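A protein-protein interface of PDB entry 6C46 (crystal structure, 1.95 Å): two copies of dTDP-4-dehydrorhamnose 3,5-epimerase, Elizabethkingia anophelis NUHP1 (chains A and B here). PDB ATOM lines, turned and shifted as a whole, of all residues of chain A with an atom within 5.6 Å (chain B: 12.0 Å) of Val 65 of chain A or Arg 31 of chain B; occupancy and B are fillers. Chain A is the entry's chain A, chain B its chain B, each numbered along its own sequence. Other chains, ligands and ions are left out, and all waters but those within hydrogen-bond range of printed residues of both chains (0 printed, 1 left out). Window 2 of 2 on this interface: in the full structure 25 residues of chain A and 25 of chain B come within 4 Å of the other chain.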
ATOM      1  N   LYS A  60      -3.080  27.280   8.211  1.00  0.00           N
ATOM      2  CA  LYS A  60      -1.760  26.681   8.347  1.00  0.00           C
ATOM      3  C   LYS A  60      -0.962  27.579   9.273  1.00  0.00           C
ATOM      4  O   LYS A  60      -0.946  28.799   9.074  1.00  0.00           O
ATOM      5  CB  LYS A  60      -1.057  26.562   7.000  1.00  0.00           C
ATOM      6  CG  LYS A  60       0.414  26.090   7.097  1.00  0.00           C
ATOM      7  CD  LYS A  60       0.946  25.603   5.748  1.00  0.00           C
ATOM      8  CE  LYS A  60       2.434  25.312   5.807  1.00  0.00           C
ATOM      9  NZ  LYS A  60       2.961  24.863   4.487  1.00  0.00           N
ATOM     10  N   SER A  61      -0.316  26.984  10.282  1.00  0.00           N
ATOM     11  CA  SER A  61       0.415  27.743  11.296  1.00  0.00           C
ATOM     12  C   SER A  61       1.653  26.960  11.689  1.00  0.00           C
ATOM     13  O   SER A  61       1.740  25.748  11.463  1.00  0.00           O
ATOM     14  CB  SER A  61      -0.449  28.021  12.544  1.00  0.00           C
ATOM     15  OG  SER A  61      -1.786  28.334  12.191  1.00  0.00           O
ATOM     16  N   SER A  62       2.613  27.654  12.292  1.00  0.00           N
ATOM     17  CA  SER A  62       3.886  27.044  12.642  1.00  0.00           C
ATOM     18  C   SER A  62       3.879  26.561  14.090  1.00  0.00           C
ATOM     19  O   SER A  62       3.000  26.912  14.880  1.00  0.00           O
ATOM     20  CB  SER A  62       5.025  28.034  12.412  1.00  0.00           C
ATOM     21  OG  SER A  62       4.981  28.511  11.086  1.00  0.00           O
ATOM     22  N   TYR A  63       4.896  25.751  14.426  1.00  0.00           N
ATOM     23  CA  TYR A  63       5.048  25.163  15.756  1.00  0.00           C
ATOM     24  C   TYR A  63       4.813  26.185  16.864  1.00  0.00           C
ATOM     25  O   TYR A  63       5.402  27.268  16.867  1.00  0.00           O
ATOM     26  CB  TYR A  63       6.459  24.557  15.919  1.00  0.00           C
ATOM     27  CG  TYR A  63       6.713  24.195  17.360  1.00  0.00           C
ATOM     28  CD1 TYR A  63       7.616  24.919  18.147  1.00  0.00           C
ATOM     29  CD2 TYR A  63       5.992  23.170  17.955  1.00  0.00           C
ATOM     30  CE1 TYR A  63       7.805  24.597  19.494  1.00  0.00           C
ATOM     31  CE2 TYR A  63       6.165  22.844  19.287  1.00  0.00           C
ATOM     32  CZ  TYR A  63       7.068  23.554  20.055  1.00  0.00           C
ATOM     33  OH  TYR A  63       7.221  23.189  21.382  1.00  0.00           O
ATOM     34  N   GLY A  64       3.962  25.832  17.816  1.00  0.00           N
ATOM     35  CA  GLY A  64       3.773  26.648  19.000  1.00  0.00           C
ATOM     36  C   GLY A  64       2.702  27.703  18.868  1.00  0.00           C
ATOM     37  O   GLY A  64       2.281  28.280  19.884  1.00  0.00           O
ATOM     38  N   VAL A  65       2.236  27.968  17.653  1.00  0.00           N
ATOM     39  CA  VAL A  65       1.095  28.859  17.495  1.00  0.00           C
ATOM     40  C   VAL A  65      -0.092  28.259  18.233  1.00  0.00           C
ATOM     41  O   VAL A  65      -0.454  27.092  18.021  1.00  0.00           O
ATOM     42  CB  VAL A  65       0.796  29.099  16.014  1.00  0.00           C
ATOM     43  CG1 VAL A  65      -0.583  29.752  15.863  1.00  0.00           C
ATOM     44  CG2 VAL A  65       1.920  30.012  15.406  1.00  0.00           C
ATOM     45  N   LEU A  66      -0.671  29.045  19.136  1.00  0.00           N
ATOM     46  CA  LEU A  66      -1.800  28.629  19.962  1.00  0.00           C
ATOM     47  C   LEU A  66      -2.921  29.636  19.750  1.00  0.00           C
ATOM     48  O   LEU A  66      -2.711  30.836  19.935  1.00  0.00           O
ATOM     49  CB  LEU A  66      -1.377  28.563  21.433  1.00  0.00           C
ATOM     50  CG  LEU A  66      -2.281  27.843  22.460  1.00  0.00           C
ATOM     51  CD1 LEU A  66      -1.477  27.531  23.700  1.00  0.00           C
ATOM     52  CD2 LEU A  66      -3.517  28.655  22.815  1.00  0.00           C
ATOM     53  N   ARG A  67      -4.088  29.161  19.302  1.00  0.00           N
ATOM     54  CA  ARG A  67      -5.243  30.011  19.027  1.00  0.00           C
ATOM     55  C   ARG A  67      -6.407  29.588  19.917  1.00  0.00           C
ATOM     56  O   ARG A  67      -6.776  28.419  19.923  1.00  0.00           O
ATOM     57  CB  ARG A  67      -5.658  29.909  17.551  1.00  0.00           C
ATOM     58  CG  ARG A  67      -4.557  30.333  16.563  1.00  0.00           C
ATOM     59  CD  ARG A  67      -4.867  31.672  15.912  1.00  0.00           C
ATOM     60  NE  ARG A  67      -3.876  32.060  14.910  1.00  0.00           N
ATOM     61  CZ  ARG A  67      -3.018  33.064  15.055  1.00  0.00           C
ATOM     62  NH1 ARG A  67      -3.021  33.778  16.173  1.00  0.00           N
ATOM     63  NH2 ARG A  67      -2.153  33.350  14.086  1.00  0.00           N
ATOM     64  N   PHE A 129      -6.616  25.500  19.825  1.00  0.00           N
ATOM     65  CA  PHE A 129      -5.638  24.460  19.535  1.00  0.00           C
ATOM     66  C   PHE A 129      -4.234  25.035  19.520  1.00  0.00           C
ATOM     67  O   PHE A 129      -4.040  26.242  19.369  1.00  0.00           O
ATOM     68  CB  PHE A 129      -5.933  23.761  18.211  1.00  0.00           C
ATOM     69  CG  PHE A 129      -5.607  24.575  16.990  1.00  0.00           C
ATOM     70  CD1 PHE A 129      -4.408  24.389  16.322  1.00  0.00           C
ATOM     71  CD2 PHE A 129      -6.519  25.486  16.479  1.00  0.00           C
ATOM     72  CE1 PHE A 129      -4.111  25.117  15.170  1.00  0.00           C
ATOM     73  CE2 PHE A 129      -6.234  26.217  15.329  1.00  0.00           C
ATOM     74  CZ  PHE A 129      -5.027  26.034  14.674  1.00  0.00           C
ATOM     75  N   VAL A 130      -3.243  24.142  19.668  1.00  0.00           N
ATOM     76  CA  VAL A 130      -1.835  24.527  19.581  1.00  0.00           C
ATOM     77  C   VAL A 130      -1.145  23.615  18.577  1.00  0.00           C
ATOM     78  O   VAL A 130      -1.483  22.431  18.467  1.00  0.00           O
ATOM     79  CB  VAL A 130      -1.133  24.440  20.953  1.00  0.00           C
ATOM     80  CG1 VAL A 130      -1.194  23.010  21.463  1.00  0.00           C
ATOM     81  CG2 VAL A 130       0.326  24.919  20.855  1.00  0.00           C
ATOM     82  N   VAL A 131      -0.214  24.172  17.807  1.00  0.00           N
ATOM     83  CA  VAL A 131       0.476  23.393  16.782  1.00  0.00           C
ATOM     84  C   VAL A 131       1.621  22.647  17.445  1.00  0.00           C
ATOM     85  O   VAL A 131       2.486  23.260  18.073  1.00  0.00           O
ATOM     86  CB  VAL A 131       0.985  24.292  15.646  1.00  0.00           C
ATOM     87  CG1 VAL A 131       1.836  23.480  14.695  1.00  0.00           C
ATOM     88  CG2 VAL A 131      -0.212  24.950  14.902  1.00  0.00           C
ATOM     89  N   ASP A 171       7.423  28.315  24.397  1.00  0.00           N
ATOM     90  CA  ASP A 171       7.251  28.037  22.973  1.00  0.00           C
ATOM     91  C   ASP A 171       5.936  28.554  22.403  1.00  0.00           C
ATOM     92  O   ASP A 171       5.793  28.587  21.175  1.00  0.00           O
ATOM     93  CB  ASP A 171       7.306  26.523  22.696  1.00  0.00           C
ATOM     94  CG  ASP A 171       8.670  25.924  22.944  1.00  0.00           C
ATOM     95  OD1 ASP A 171       9.591  26.686  23.270  1.00  0.00           O
ATOM     96  OD2 ASP A 171       8.827  24.697  22.777  1.00  0.00           O
ATOM     97  N   MET A 172       4.979  28.953  23.241  1.00  0.00           N
ATOM     98  CA  MET A 172       3.652  29.307  22.743  1.00  0.00           C
ATOM     99  C   MET A 172       3.678  30.684  22.091  1.00  0.00           C
ATOM    100  O   MET A 172       4.300  31.624  22.600  1.00  0.00           O
ATOM    101  CB  MET A 172       2.627  29.273  23.877  1.00  0.00           C
ATOM    102  CG  MET A 172       2.489  27.913  24.524  1.00  0.00           C
ATOM    103  SD  MET A 172       1.560  28.010  26.073  1.00  0.00           S
ATOM    104  CE  MET A 172       1.660  26.314  26.660  1.00  0.00           C
ATOM    105  N   ILE A 173       3.009  30.794  20.948  1.00  0.00           N
ATOM    106  CA  ILE A 173       2.899  32.039  20.199  1.00  0.00           C
ATOM    107  C   ILE A 173       1.430  32.445  20.181  1.00  0.00           C
ATOM    108  O   ILE A 173       0.598  31.739  19.600  1.00  0.00           O
ATOM    109  CB  ILE A 173       3.444  31.879  18.772  1.00  0.00           C
ATOM    110  CG1 ILE A 173       4.917  31.444  18.816  1.00  0.00           C
ATOM    111  CG2 ILE A 173       3.234  33.159  17.978  1.00  0.00           C
ATOM    112  CD1 ILE A 173       5.475  31.050  17.452  1.00  0.00           C
ATOM    113  N   VAL B  26      -6.784  33.836  -0.070  1.00  0.00           N
ATOM    114  CA  VAL B  26      -5.888  33.310   0.952  1.00  0.00           C
ATOM    115  C   VAL B  26      -5.230  34.488   1.637  1.00  0.00           C
ATOM    116  O   VAL B  26      -4.606  35.329   0.980  1.00  0.00           O
ATOM    117  CB  VAL B  26      -4.836  32.361   0.354  1.00  0.00           C
ATOM    118  CG1 VAL B  26      -3.937  31.810   1.470  1.00  0.00           C
ATOM    119  CG2 VAL B  26      -5.512  31.233  -0.392  1.00  0.00           C
ATOM    120  N   PHE B  27      -5.381  34.557   2.950  1.00  0.00           N
ATOM    121  CA  PHE B  27      -4.752  35.594   3.749  1.00  0.00           C
ATOM    122  C   PHE B  27      -3.477  35.028   4.344  1.00  0.00           C
ATOM    123  O   PHE B  27      -3.526  34.036   5.079  1.00  0.00           O
ATOM    124  CB  PHE B  27      -5.708  36.082   4.839  1.00  0.00           C
ATOM    125  CG  PHE B  27      -6.974  36.665   4.283  1.00  0.00           C
ATOM    126  CD1 PHE B  27      -8.088  35.861   4.070  1.00  0.00           C
ATOM    127  CD2 PHE B  27      -7.030  38.000   3.901  1.00  0.00           C
ATOM    128  CE1 PHE B  27      -9.254  36.389   3.527  1.00  0.00           C
ATOM    129  CE2 PHE B  27      -8.190  38.537   3.359  1.00  0.00           C
ATOM    130  CZ  PHE B  27      -9.304  37.729   3.168  1.00  0.00           C
ATOM    131  N   GLU B  28      -2.343  35.657   4.042  1.00  0.00           N
ATOM    132  CA  GLU B  28      -1.063  35.180   4.540  1.00  0.00           C
ATOM    133  C   GLU B  28      -0.682  36.042   5.738  1.00  0.00           C
ATOM    134  O   GLU B  28      -1.096  37.198   5.852  1.00  0.00           O
ATOM    135  CB  GLU B  28       0.025  35.244   3.461  1.00  0.00           C
ATOM    136  CG  GLU B  28      -0.227  34.335   2.250  1.00  0.00           C
ATOM    137  CD  GLU B  28       0.595  33.048   2.276  1.00  0.00           C
ATOM    138  OE1 GLU B  28       1.438  32.897   3.184  1.00  0.00           O
ATOM    139  OE2 GLU B  28       0.404  32.184   1.388  1.00  0.00           O
ATOM    140  N   ASP B  29       0.101  35.467   6.642  1.00  0.00           N
ATOM    141  CA  ASP B  29       0.502  36.185   7.844  1.00  0.00           C
ATOM    142  C   ASP B  29       1.860  35.671   8.299  1.00  0.00           C
ATOM    143  O   ASP B  29       2.536  34.929   7.578  1.00  0.00           O
ATOM    144  CB  ASP B  29      -0.564  36.030   8.940  1.00  0.00           C
ATOM    145  CG  ASP B  29      -0.945  34.570   9.188  1.00  0.00           C
ATOM    146  OD1 ASP B  29      -0.369  33.939  10.101  1.00  0.00           O
ATOM    147  OD2 ASP B  29      -1.820  34.048   8.465  1.00  0.00           O
ATOM    148  N   GLU B  30       2.244  36.070   9.516  1.00  0.00           N
ATOM    149  CA  GLU B  30       3.549  35.705  10.060  1.00  0.00           C
ATOM    150  C   GLU B  30       3.671  34.194  10.229  1.00  0.00           C
ATOM    151  O   GLU B  30       4.679  33.590   9.841  1.00  0.00           O
ATOM    152  CB  GLU B  30       3.772  36.422  11.394  1.00  0.00           C
ATOM    153  N   ARG B  31       2.637  33.561  10.786  1.00  0.00           N
ATOM    154  CA  ARG B  31       2.702  32.138  11.095  1.00  0.00           C
ATOM    155  C   ARG B  31       2.275  31.230   9.945  1.00  0.00           C
ATOM    156  O   ARG B  31       2.476  30.017  10.045  1.00  0.00           O
ATOM    157  CB  ARG B  31       1.810  31.838  12.308  1.00  0.00           C
ATOM    158  N   GLY B  32       1.758  31.765   8.837  1.00  0.00           N
ATOM    159  CA  GLY B  32       1.166  30.887   7.838  1.00  0.00           C
ATOM    160  C   GLY B  32       0.095  31.549   6.989  1.00  0.00           C
ATOM    161  O   GLY B  32       0.362  32.555   6.322  1.00  0.00           O
ATOM    162  N   TYR B  33      -1.107  30.966   6.960  1.00  0.00           N
ATOM    163  CA  TYR B  33      -2.205  31.534   6.188  1.00  0.00           C
ATOM    164  C   TYR B  33      -3.543  31.036   6.737  1.00  0.00           C
ATOM    165  O   TYR B  33      -3.612  30.113   7.557  1.00  0.00           O
ATOM    166  CB  TYR B  33      -2.068  31.193   4.692  1.00  0.00           C
ATOM    167  CG  TYR B  33      -2.191  29.717   4.331  1.00  0.00           C
ATOM    168  CD1 TYR B  33      -3.411  29.056   4.422  1.00  0.00           C
ATOM    169  CD2 TYR B  33      -1.092  28.991   3.890  1.00  0.00           C
ATOM    170  CE1 TYR B  33      -3.530  27.720   4.121  1.00  0.00           C
ATOM    171  CE2 TYR B  33      -1.214  27.638   3.557  1.00  0.00           C
ATOM    172  CZ  TYR B  33      -2.432  27.012   3.676  1.00  0.00           C
ATOM    173  OH  TYR B  33      -2.587  25.670   3.368  1.00  0.00           O
ATOM    174  N   PHE B  34      -4.614  31.663   6.262  1.00  0.00           N
ATOM    175  CA  PHE B  34      -5.944  31.122   6.496  1.00  0.00           C
ATOM    176  C   PHE B  34      -6.850  31.517   5.347  1.00  0.00           C
ATOM    177  O   PHE B  34      -6.644  32.551   4.710  1.00  0.00           O
ATOM    178  CB  PHE B  34      -6.535  31.611   7.810  1.00  0.00           C
ATOM    179  CG  PHE B  34      -6.492  33.095   7.978  1.00  0.00           C
ATOM    180  CD1 PHE B  34      -7.595  33.872   7.656  1.00  0.00           C
ATOM    181  CD2 PHE B  34      -5.348  33.721   8.475  1.00  0.00           C
ATOM    182  CE1 PHE B  34      -7.560  35.258   7.820  1.00  0.00           C
ATOM    183  CE2 PHE B  34      -5.300  35.100   8.642  1.00  0.00           C
ATOM    184  CZ  PHE B  34      -6.409  35.870   8.316  1.00  0.00           C
ATOM    185  N   TYR B  35      -7.872  30.701   5.110  1.00  0.00           N
ATOM    186  CA  TYR B  35      -8.893  31.074   4.146  1.00  0.00           C
ATOM    187  C   TYR B  35     -10.185  30.338   4.451  1.00  0.00           C
ATOM    188  O   TYR B  35     -10.202  29.286   5.114  1.00  0.00           O
ATOM    189  CB  TYR B  35      -8.460  30.810   2.710  1.00  0.00           C
ATOM    190  CG  TYR B  35      -8.185  29.375   2.343  1.00  0.00           C
ATOM    191  CD1 TYR B  35      -9.115  28.625   1.613  1.00  0.00           C
ATOM    192  CD2 TYR B  35      -6.964  28.788   2.657  1.00  0.00           C
ATOM    193  CE1 TYR B  35      -8.833  27.314   1.237  1.00  0.00           C
ATOM    194  CE2 TYR B  35      -6.682  27.482   2.285  1.00  0.00           C
ATOM    195  CZ  TYR B  35      -7.610  26.760   1.590  1.00  0.00           C
ATOM    196  OH  TYR B  35      -7.322  25.478   1.237  1.00  0.00           O
ATOM    197  N   LYS B 116      -4.728  24.780  -4.101  1.00  0.00           N
ATOM    198  CA  LYS B 116      -5.866  24.931  -3.194  1.00  0.00           C
ATOM    199  C   LYS B 116      -7.192  25.119  -3.920  1.00  0.00           C
ATOM    200  O   LYS B 116      -8.169  25.570  -3.313  1.00  0.00           O
ATOM    201  CB  LYS B 116      -5.647  26.112  -2.232  1.00  0.00           C
ATOM    202  CG  LYS B 116      -4.337  26.068  -1.421  1.00  0.00           C
ATOM    203  CD  LYS B 116      -4.203  27.387  -0.614  1.00  0.00           C
ATOM    204  CE  LYS B 116      -2.828  27.558   0.056  1.00  0.00           C
ATOM    205  NZ  LYS B 116      -1.711  27.632  -0.929  1.00  0.00           N
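Of chain B, only Arg 31 (3.6 Å) comes within 4 Å of Val 65 of chain A.
Printed residues of chain A within 4 Å of Arg 31 of chain B: Lys 60, Ser 61, Ser 62 and Val 65.
Lys 60 of chain A touches three residues of chain B.
Of the printed residues of chain B, Ser 61 of chain A touches Arg 31.
No residue of chain B comes within 4 Å of Gly 64 of chain A.
No residue of chain B comes within 4 Å of Leu 66 of chain A.
No residue of chain B comes within 4 Å of Phe 129 of chain A.
No residue of chain B comes within 4 Å of Val 131 of chain A.
No residue of chain B comes within 4 Å of Ile 173 of chain A.
Of the printed residues of chain A, Tyr 33 of chain B touches Lys 60 (3.0 Å).
Of the printed residues of chain B, Ser 62 of chain A touches Arg 31 (3.1 Å).
Of the printed residues of chain A, Gly 32 of chain B touches Lys 60 (3.2 Å).
The nearest printed residue of chain A that does not touch Arg 31 of chain B is Arg 67 of chain A (4.6 Å).
The nearest printed residue of chain A that does not touch Tyr 33 of chain B is Ser 61 of chain A (5.2 Å).
Of the 11 printed residues of chain B, 3 touch a printed residue of chain A.
Printed residues of chain B that touch a printed residue of chain A: Arg 31, Gly 32 and Tyr 33.
Hydrophobic or aromatic side chains of chain B within 4 Å of the printed part of chain A: Tyr 33.
Of the 14 printed residues of chain A, 4 touch a printed residue of chain B.
Among the printed residues, no Asp or Glu carboxylate lies within 4 Å of a Lys or Arg side-chain nitrogen of the other chain.
No position is printed for both chains.
Of the 6 pairs that touch across the chains among the printed residues, none has its exchanged pair printed and touching as well.
The backbone carbonyl oxygen (O) of Tyr 33 of chain B is in hydrogen-bond range of the backbone NH (N) of Lys 60 of chain A (3.0 Å).
The side-chain hydroxyl of Ser 62 of chain A lies within hydrogen-bond range of the backbone carbonyl oxygen of Arg 31 of chain B, 3.1 Å away.
Among the printed residues, pairs that only touch across the chains: Lys 60 of chain A with Arg 31 of chain B, Lys 60 of chain A with Gly 32 of chain B, Ser 61 of chain A with Arg 31 of chain B and Val 65 of chain A with Arg 31 of chain B.
The backbone carbonyl oxygen (O) of Val 65 of chain A lies within hydrogen-bond range of the backbone NH (N) of Val 131 of chain A.
The side-chain carboxylate (OD1) of Asp 29 of chain B sits at hydrogen-bond distance from the backbone NH (N) of Arg 31 of chain B (3.1 Å).
The side-chain carboxylate of Asp 29 of chain B is in hydrogen-bond range of the backbone NH of Gly 32 of chain B, 3.3 Å away.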
